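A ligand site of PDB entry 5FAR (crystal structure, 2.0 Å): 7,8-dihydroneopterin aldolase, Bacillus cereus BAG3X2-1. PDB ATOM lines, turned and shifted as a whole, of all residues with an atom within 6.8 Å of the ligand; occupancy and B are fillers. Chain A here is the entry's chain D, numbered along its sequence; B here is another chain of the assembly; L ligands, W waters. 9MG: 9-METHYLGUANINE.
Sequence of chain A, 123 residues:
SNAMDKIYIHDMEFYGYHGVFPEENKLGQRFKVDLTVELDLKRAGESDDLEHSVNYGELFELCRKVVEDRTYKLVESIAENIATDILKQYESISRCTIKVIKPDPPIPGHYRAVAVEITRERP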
ATOM      1  N   ILE A   7      10.511 -14.223 -21.236  1.00  0.00           N
ATOM      2  CA  ILE A   7       9.886 -15.319 -20.476  1.00  0.00           C
ATOM      3  C   ILE A   7      10.975 -15.878 -19.554  1.00  0.00           C
ATOM      4  O   ILE A   7      12.048 -16.229 -20.012  1.00  0.00           O
ATOM      5  CB  ILE A   7       9.325 -16.441 -21.372  1.00  0.00           C
ATOM      6  CG1 ILE A   7       8.259 -15.883 -22.324  1.00  0.00           C
ATOM      7  CG2 ILE A   7       8.695 -17.563 -20.531  1.00  0.00           C
ATOM      8  CD1 ILE A   7       7.752 -16.874 -23.339  1.00  0.00           C
ATOM      9  N   LEU A  41       6.547  -9.965 -27.117  1.00  0.00           N
ATOM     10  CA  LEU A  41       5.338 -10.531 -26.524  1.00  0.00           C
ATOM     11  C   LEU A  41       4.141  -9.580 -26.613  1.00  0.00           C
ATOM     12  O   LEU A  41       3.099  -9.847 -26.022  1.00  0.00           O
ATOM     13  CB  LEU A  41       5.634 -10.932 -25.061  1.00  0.00           C
ATOM     14  CG  LEU A  41       6.883 -11.829 -24.917  1.00  0.00           C
ATOM     15  CD1 LEU A  41       7.428 -11.888 -23.510  1.00  0.00           C
ATOM     16  CD2 LEU A  41       6.587 -13.224 -25.449  1.00  0.00           C
ATOM     17  N   ASP A  48      -3.954 -12.563 -27.051  1.00  0.00           N
ATOM     18  CA  ASP A  48      -4.054 -13.611 -26.031  1.00  0.00           C
ATOM     19  C   ASP A  48      -3.830 -14.980 -26.684  1.00  0.00           C
ATOM     20  O   ASP A  48      -4.399 -15.987 -26.260  1.00  0.00           O
ATOM     21  CB  ASP A  48      -5.418 -13.545 -25.295  1.00  0.00           C
ATOM     22  CG  ASP A  48      -5.372 -14.152 -23.901  1.00  0.00           C
ATOM     23  OD1 ASP A  48      -4.270 -14.289 -23.325  1.00  0.00           O
ATOM     24  OD2 ASP A  48      -6.448 -14.482 -23.365  1.00  0.00           O
ATOM     25  N   LEU A  50      -1.285 -17.954 -27.736  1.00  0.00           N
ATOM     26  CA  LEU A  50      -0.037 -18.640 -27.390  1.00  0.00           C
ATOM     27  C   LEU A  50       0.889 -18.932 -28.583  1.00  0.00           C
ATOM     28  O   LEU A  50       2.101 -19.051 -28.406  1.00  0.00           O
ATOM     29  CB  LEU A  50      -0.358 -19.971 -26.680  1.00  0.00           C
ATOM     30  CG  LEU A  50       0.788 -20.855 -26.176  1.00  0.00           C
ATOM     31  CD1 LEU A  50       1.651 -20.090 -25.172  1.00  0.00           C
ATOM     32  CD2 LEU A  50       0.243 -22.140 -25.561  1.00  0.00           C
ATOM     33  N   SER A  53       3.492 -16.348 -29.004  1.00  0.00           N
ATOM     34  CA  SER A  53       4.445 -16.570 -27.924  1.00  0.00           C
ATOM     35  C   SER A  53       5.012 -18.000 -27.980  1.00  0.00           C
ATOM     36  O   SER A  53       5.029 -18.627 -29.030  1.00  0.00           O
ATOM     37  CB  SER A  53       3.787 -16.284 -26.579  1.00  0.00           C
ATOM     38  OG  SER A  53       4.795 -15.999 -25.622  1.00  0.00           O
ATOM     39  N   VAL A  54       5.480 -18.495 -26.828  1.00  0.00           N
ATOM     40  CA  VAL A  54       6.143 -19.788 -26.706  1.00  0.00           C
ATOM     41  C   VAL A  54       5.673 -20.482 -25.420  1.00  0.00           C
ATOM     42  O   VAL A  54       5.722 -19.880 -24.348  1.00  0.00           O
ATOM     43  CB  VAL A  54       7.685 -19.607 -26.668  1.00  0.00           C
ATOM     44  CG1 VAL A  54       8.398 -20.903 -26.278  1.00  0.00           C
ATOM     45  CG2 VAL A  54       8.186 -19.085 -28.006  1.00  0.00           C
ATOM     46  N   ASN A  55       5.204 -21.720 -25.563  1.00  0.00           N
ATOM     47  CA  ASN A  55       4.893 -22.608 -24.431  1.00  0.00           C
ATOM     48  C   ASN A  55       5.980 -22.610 -23.343  1.00  0.00           C
ATOM     49  O   ASN A  55       7.132 -22.977 -23.617  1.00  0.00           O
ATOM     50  CB  ASN A  55       4.658 -24.037 -24.962  1.00  0.00           C
ATOM     51  CG  ASN A  55       3.859 -24.924 -24.006  1.00  0.00           C
ATOM     52  OD1 ASN A  55       4.130 -24.967 -22.808  1.00  0.00           O
ATOM     53  ND2 ASN A  55       2.878 -25.657 -24.530  1.00  0.00           N
ATOM     54  N   TYR A  56       5.629 -22.186 -22.116  1.00  0.00           N
ATOM     55  CA  TYR A  56       6.586 -22.257 -20.998  1.00  0.00           C
ATOM     56  C   TYR A  56       6.881 -23.707 -20.631  1.00  0.00           C
ATOM     57  O   TYR A  56       7.973 -24.012 -20.183  1.00  0.00           O
ATOM     58  CB  TYR A  56       6.214 -21.357 -19.779  1.00  0.00           C
ATOM     59  CG  TYR A  56       4.844 -21.532 -19.091  1.00  0.00           C
ATOM     60  CD1 TYR A  56       4.417 -22.774 -18.616  1.00  0.00           C
ATOM     61  CD2 TYR A  56       4.005 -20.438 -18.859  1.00  0.00           C
ATOM     62  CE1 TYR A  56       3.186 -22.925 -17.959  1.00  0.00           C
ATOM     63  CE2 TYR A  56       2.780 -20.579 -18.218  1.00  0.00           C
ATOM     64  CZ  TYR A  56       2.370 -21.835 -17.770  1.00  0.00           C
ATOM     65  OH  TYR A  56       1.142 -21.982 -17.135  1.00  0.00           O
ATOM     66  N   GLY A  57       5.928 -24.607 -20.865  1.00  0.00           N
ATOM     67  CA  GLY A  57       6.080 -26.027 -20.510  1.00  0.00           C
ATOM     68  C   GLY A  57       7.096 -26.743 -21.369  1.00  0.00           C
ATOM     69  O   GLY A  57       8.003 -27.397 -20.882  1.00  0.00           O
ATOM     70  N   GLU A  58       6.965 -26.575 -22.682  1.00  0.00           N
ATOM     71  CA  GLU A  58       7.960 -27.125 -23.603  1.00  0.00           C
ATOM     72  C   GLU A  58       9.365 -26.644 -23.282  1.00  0.00           C
ATOM     73  O   GLU A  58      10.330 -27.385 -23.472  1.00  0.00           O
ATOM     74  CB  GLU A  58       7.608 -26.762 -25.037  1.00  0.00           C
ATOM     75  CG  GLU A  58       6.402 -27.469 -25.632  1.00  0.00           C
ATOM     76  CD  GLU A  58       6.056 -26.929 -27.009  1.00  0.00           C
ATOM     77  OE1 GLU A  58       6.991 -26.593 -27.760  1.00  0.00           O
ATOM     78  OE2 GLU A  58       4.856 -26.814 -27.336  1.00  0.00           O
ATOM     79  N   LEU A  59       9.493 -25.409 -22.808  1.00  0.00           N
ATOM     80  CA  LEU A  59      10.789 -24.874 -22.367  1.00  0.00           C
ATOM     81  C   LEU A  59      11.351 -25.672 -21.189  1.00  0.00           C
ATOM     82  O   LEU A  59      12.529 -26.023 -21.203  1.00  0.00           O
ATOM     83  CB  LEU A  59      10.676 -23.397 -21.989  1.00  0.00           C
ATOM     84  CG  LEU A  59      10.775 -22.354 -23.102  1.00  0.00           C
ATOM     85  CD1 LEU A  59      10.367 -20.990 -22.560  1.00  0.00           C
ATOM     86  CD2 LEU A  59      12.168 -22.301 -23.697  1.00  0.00           C
ATOM     87  N   HIS B  18      -6.749 -17.426 -14.429  1.00  0.00           N
ATOM     88  CA  HIS B  18      -6.256 -17.208 -15.808  1.00  0.00           C
ATOM     89  C   HIS B  18      -5.544 -18.438 -16.331  1.00  0.00           C
ATOM     90  O   HIS B  18      -4.726 -19.018 -15.628  1.00  0.00           O
ATOM     91  CB  HIS B  18      -5.211 -16.074 -15.900  1.00  0.00           C
ATOM     92  CG  HIS B  18      -5.574 -14.809 -15.206  1.00  0.00           C
ATOM     93  ND1 HIS B  18      -5.787 -13.632 -15.884  1.00  0.00           N
ATOM     94  CD2 HIS B  18      -5.709 -14.508 -13.888  1.00  0.00           C
ATOM     95  CE1 HIS B  18      -6.056 -12.664 -15.022  1.00  0.00           C
ATOM     96  NE2 HIS B  18      -6.023 -13.177 -13.811  1.00  0.00           N
ATOM     97  N   GLY B  19      -5.762 -18.793 -17.582  1.00  0.00           N
ATOM     98  CA  GLY B  19      -4.975 -19.869 -18.163  1.00  0.00           C
ATOM     99  C   GLY B  19      -5.384 -20.347 -19.532  1.00  0.00           C
ATOM    100  O   GLY B  19      -6.486 -20.040 -20.009  1.00  0.00           O
ATOM    101  N   VAL B  20      -4.473 -21.096 -20.139  1.00  0.00           N
ATOM    102  CA  VAL B  20      -4.699 -21.777 -21.420  1.00  0.00           C
ATOM    103  C   VAL B  20      -5.675 -22.950 -21.276  1.00  0.00           C
ATOM    104  O   VAL B  20      -6.536 -23.130 -22.132  1.00  0.00           O
ATOM    105  CB  VAL B  20      -3.354 -22.202 -22.061  1.00  0.00           C
ATOM    106  CG1 VAL B  20      -3.561 -23.113 -23.271  1.00  0.00           C
ATOM    107  CG2 VAL B  20      -2.563 -20.960 -22.483  1.00  0.00           C
ATOM    108  N   PHE B  21      -5.528 -23.736 -20.201  1.00  0.00           N
ATOM    109  CA  PHE B  21      -6.412 -24.881 -19.915  1.00  0.00           C
ATOM    110  C   PHE B  21      -7.723 -24.457 -19.262  1.00  0.00           C
ATOM    111  O   PHE B  21      -7.697 -23.637 -18.345  1.00  0.00           O
ATOM    112  CB  PHE B  21      -5.752 -25.861 -18.933  1.00  0.00           C
ATOM    113  CG  PHE B  21      -4.473 -26.480 -19.425  1.00  0.00           C
ATOM    114  CD1 PHE B  21      -4.399 -27.072 -20.681  1.00  0.00           C
ATOM    115  CD2 PHE B  21      -3.367 -26.539 -18.594  1.00  0.00           C
ATOM    116  CE1 PHE B  21      -3.224 -27.673 -21.113  1.00  0.00           C
ATOM    117  CE2 PHE B  21      -2.189 -27.133 -19.019  1.00  0.00           C
ATOM    118  CZ  PHE B  21      -2.113 -27.703 -20.286  1.00  0.00           C
ATOM    119  N   GLU B  24      -7.546 -24.944 -15.471  1.00  0.00           N
ATOM    120  CA  GLU B  24      -7.010 -23.730 -14.814  1.00  0.00           C
ATOM    121  C   GLU B  24      -8.068 -22.680 -14.544  1.00  0.00           C
ATOM    122  O   GLU B  24      -8.106 -22.092 -13.453  1.00  0.00           O
ATOM    123  CB  GLU B  24      -5.861 -23.115 -15.625  1.00  0.00           C
ATOM    124  CG  GLU B  24      -4.626 -23.984 -15.669  1.00  0.00           C
ATOM    125  CD  GLU B  24      -3.415 -23.267 -16.224  1.00  0.00           C
ATOM    126  OE1 GLU B  24      -3.274 -23.265 -17.466  1.00  0.00           O
ATOM    127  OE2 GLU B  24      -2.601 -22.742 -15.424  1.00  0.00           O
ATOM    128  N   LYS B  73      -6.307 -15.805 -20.960  1.00  0.00           N
ATOM    129  CA  LYS B  73      -5.636 -17.094 -21.110  1.00  0.00           C
ATOM    130  C   LYS B  73      -4.133 -16.995 -20.839  1.00  0.00           C
ATOM    131  O   LYS B  73      -3.559 -17.916 -20.267  1.00  0.00           O
ATOM    132  CB  LYS B  73      -5.903 -17.687 -22.500  1.00  0.00           C
ATOM    133  CG  LYS B  73      -7.356 -18.104 -22.684  1.00  0.00           C
ATOM    134  CD  LYS B  73      -7.703 -18.329 -24.151  1.00  0.00           C
ATOM    135  CE  LYS B  73      -9.216 -18.300 -24.366  1.00  0.00           C
ATOM    136  NZ  LYS B  73      -9.742 -16.905 -24.493  1.00  0.00           N
ATOM    137  N   LEU B  74      -3.511 -15.892 -21.242  1.00  0.00           N
ATOM    138  CA  LEU B  74      -2.067 -15.738 -21.097  1.00  0.00           C
ATOM    139  C   LEU B  74      -1.681 -14.697 -20.032  1.00  0.00           C
ATOM    140  O   LEU B  74      -2.242 -13.585 -19.994  1.00  0.00           O
ATOM    141  CB  LEU B  74      -1.426 -15.377 -22.436  1.00  0.00           C
ATOM    142  CG  LEU B  74      -1.658 -16.292 -23.659  1.00  0.00           C
ATOM    143  CD1 LEU B  74      -0.654 -15.947 -24.742  1.00  0.00           C
ATOM    144  CD2 LEU B  74      -1.586 -17.775 -23.313  1.00  0.00           C
ATOM    145  N   VAL B  75      -0.711 -15.061 -19.178  1.00  0.00           N
ATOM    146  CA  VAL B  75       0.000 -14.081 -18.344  1.00  0.00           C
ATOM    147  C   VAL B  75       0.643 -12.956 -19.165  1.00  0.00           C
ATOM    148  O   VAL B  75       0.908 -11.885 -18.619  1.00  0.00           O
ATOM    149  CB  VAL B  75       1.085 -14.731 -17.445  1.00  0.00           C
ATOM    150  CG1 VAL B  75       0.469 -15.698 -16.445  1.00  0.00           C
ATOM    151  CG2 VAL B  75       2.184 -15.418 -18.240  1.00  0.00           C
ATOM    152  N   GLU B  76       0.905 -13.192 -20.453  1.00  0.00           N
ATOM    153  CA  GLU B  76       1.279 -12.122 -21.390  1.00  0.00           C
ATOM    154  C   GLU B  76       0.204 -11.037 -21.544  1.00  0.00           C
ATOM    155  O   GLU B  76       0.565  -9.884 -21.827  1.00  0.00           O
ATOM    156  CB  GLU B  76       1.622 -12.688 -22.777  1.00  0.00           C
ATOM    157  CG  GLU B  76       2.954 -13.425 -22.886  1.00  0.00           C
ATOM    158  CD  GLU B  76       2.825 -14.926 -22.692  1.00  0.00           C
ATOM    159  OE1 GLU B  76       2.081 -15.346 -21.797  1.00  0.00           O
ATOM    160  OE2 GLU B  76       3.479 -15.691 -23.435  1.00  0.00           O
ATOM    161  N   SER B  77      -1.071 -11.389 -21.403  1.00  0.00           N
ATOM    162  CA  SER B  77      -2.159 -10.405 -21.465  1.00  0.00           C
ATOM    163  C   SER B  77      -2.346  -9.643 -20.153  1.00  0.00           C
ATOM    164  O   SER B  77      -2.778  -8.487 -20.162  1.00  0.00           O
ATOM    165  CB  SER B  77      -3.473 -11.054 -21.862  1.00  0.00           C
ATOM    166  OG  SER B  77      -3.330 -11.768 -23.071  1.00  0.00           O
ATOM    167  N   LYS B 102       3.718 -16.903 -12.251  1.00  0.00           N
ATOM    168  CA  LYS B 102       2.825 -18.006 -12.042  1.00  0.00           C
ATOM    169  C   LYS B 102       3.623 -18.988 -11.159  1.00  0.00           C
ATOM    170  O   LYS B 102       4.280 -19.883 -11.671  1.00  0.00           O
ATOM    171  CB  LYS B 102       2.414 -18.611 -13.394  1.00  0.00           C
ATOM    172  CG  LYS B 102       0.912 -18.826 -13.565  1.00  0.00           C
ATOM    173  CD  LYS B 102       0.590 -19.876 -14.610  1.00  0.00           C
ATOM    174  CE  LYS B 102      -0.793 -19.730 -15.189  1.00  0.00           C
ATOM    175  NZ  LYS B 102      -1.040 -20.729 -16.272  1.00  0.00           N
ATOM    176  N   PRO B 106       0.618 -25.661 -13.847  1.00  0.00           N
ATOM    177  CA  PRO B 106       0.412 -27.085 -13.973  1.00  0.00           C
ATOM    178  C   PRO B 106       1.424 -27.847 -14.776  1.00  0.00           C
ATOM    179  O   PRO B 106       1.034 -28.641 -15.628  1.00  0.00           O
ATOM    180  CB  PRO B 106      -0.983 -27.167 -14.594  1.00  0.00           C
ATOM    181  CG  PRO B 106      -1.129 -25.873 -15.333  1.00  0.00           C
ATOM    182  CD  PRO B 106      -0.554 -24.925 -14.345  1.00  0.00           C
ATOM    183  N   ILE B 107       2.709 -27.684 -14.459  1.00  0.00           N
ATOM    184  CA  ILE B 107       3.780 -28.398 -15.158  1.00  0.00           C
ATOM    185  C   ILE B 107       4.443 -29.458 -14.316  1.00  0.00           C
ATOM    186  O   ILE B 107       4.929 -29.143 -13.251  1.00  0.00           O
ATOM    187  CB  ILE B 107       4.935 -27.490 -15.584  1.00  0.00           C
ATOM    188  CG1 ILE B 107       4.425 -26.341 -16.459  1.00  0.00           C
ATOM    189  CG2 ILE B 107       6.007 -28.307 -16.312  1.00  0.00           C
ATOM    190  CD1 ILE B 107       5.434 -25.232 -16.582  1.00  0.00           C
ATOM    191  N   VAL B 116       6.465 -13.894 -17.084  1.00  0.00           N
ATOM    192  CA  VAL B 116       6.653 -13.022 -18.237  1.00  0.00           C
ATOM    193  C   VAL B 116       7.090 -11.702 -17.674  1.00  0.00           C
ATOM    194  O   VAL B 116       6.882 -11.435 -16.470  1.00  0.00           O
ATOM    195  CB  VAL B 116       5.387 -12.862 -19.101  1.00  0.00           C
ATOM    196  CG1 VAL B 116       5.129 -14.136 -19.878  1.00  0.00           C
ATOM    197  CG2 VAL B 116       4.163 -12.500 -18.266  1.00  0.00           C
HETATM  198  C1  9MG L   1       1.804 -23.424 -21.546  1.00  0.00           C
HETATM  199  N2  9MG L   1       1.220 -22.134 -21.122  1.00  0.00           N
HETATM  200  C3  9MG L   1       0.055 -22.002 -20.454  1.00  0.00           C
HETATM  201  N4  9MG L   1      -0.206 -20.692 -20.220  1.00  0.00           N
HETATM  202  C5  9MG L   1       0.815 -19.968 -20.731  1.00  0.00           C
HETATM  203  C6  9MG L   1       1.191 -18.533 -20.821  1.00  0.00           C
HETATM  204  O7  9MG L   1       0.403 -17.565 -20.311  1.00  0.00           O
HETATM  205  N8  9MG L   1       2.340 -18.199 -21.440  1.00  0.00           N
HETATM  206  C9  9MG L   1       3.163 -19.125 -21.971  1.00  0.00           C
HETATM  207  N10 9MG L   1       4.299 -18.690 -22.565  1.00  0.00           N
HETATM  208  N11 9MG L   1       2.886 -20.465 -21.918  1.00  0.00           N
HETATM  209  C12 9MG L   1       1.757 -20.929 -21.327  1.00  0.00           C
HETATM  210  O   HOH W   1      -0.739 -18.673 -18.148  1.00  0.00           O
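The side-chain amide oxygen (OD1) of Asn 55 is in hydrogen-bond range of the backbone NH (N) of Gly 57, 2.7 Å away.
The side-chain hydroxyl (OG) of Ser 53 lies within hydrogen-bond range of the side-chain carboxylate (OE2) of Glu 76 of chain B, at 2.6 Å.
The backbone NH (N) of Leu 74 of chain B lies within hydrogen-bond range of the side-chain carboxylate (OD1) of Asp 48 (2.7 Å).
N of Glu 58 sits at hydrogen-bond distance from OD1 of Asn 55 (3.3 Å).
O of Lys 73 of chain B is in hydrogen-bond range of N of Val 20 of chain B (3.3 Å).
The backbone NH of Lys 73 of chain B sits at hydrogen-bond distance from the side-chain carboxylate of Asp 48, at 2.7 Å.
The side-chain hydroxyl (OH) of Tyr 56 lies within hydrogen-bond range of the side-chain amino group (NZ) of Lys 102 of chain B, 2.7 Å away.
Ile 7 touches the ligand (CD1 to N10, 3.98 Å).
CD1 of Leu 50 touches N11 of the ligand, at 3.5 Å.
Asn 55 touches the ligand.
CG2 of Val 20 of chain B touches N4 of the ligand (3.3 Å).
Lys 73 of chain B touches the ligand.
CA of Leu 74 of chain B touches O7 of the ligand, at 3.2 Å.
Hydrophobic or aromatic side chains within 4 Å of the ligand: Ile 7, Leu 50, Tyr 56, Val 20 of chain B, Leu 74 of chain B and Val 75 of chain B.
Of the 25 residues printed, 10 come within 4 Å of the ligand.
The nearest printed residue that does not touch the ligand is Lys 102 of chain B (4.04 Å).
Water W1 lies within hydrogen-bond range of an oxygen (O7) of the ligand (2.7 Å) and the side-chain amino group of Lys 102 of chain B (2.8 Å).
A nitrogen (N10) of the ligand sits at hydrogen-bond distance from the backbone carbonyl oxygen (O) of Val 54.
OE1 of Glu 76 of chain B is in hydrogen-bond range of N8 of the ligand, at 2.9 Å.
The backbone NH of Val 75 of chain B lies within hydrogen-bond range of an oxygen (O7) of the ligand.
N11 of the ligand is in hydrogen-bond range of N of Tyr 56, at 3.2 Å.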
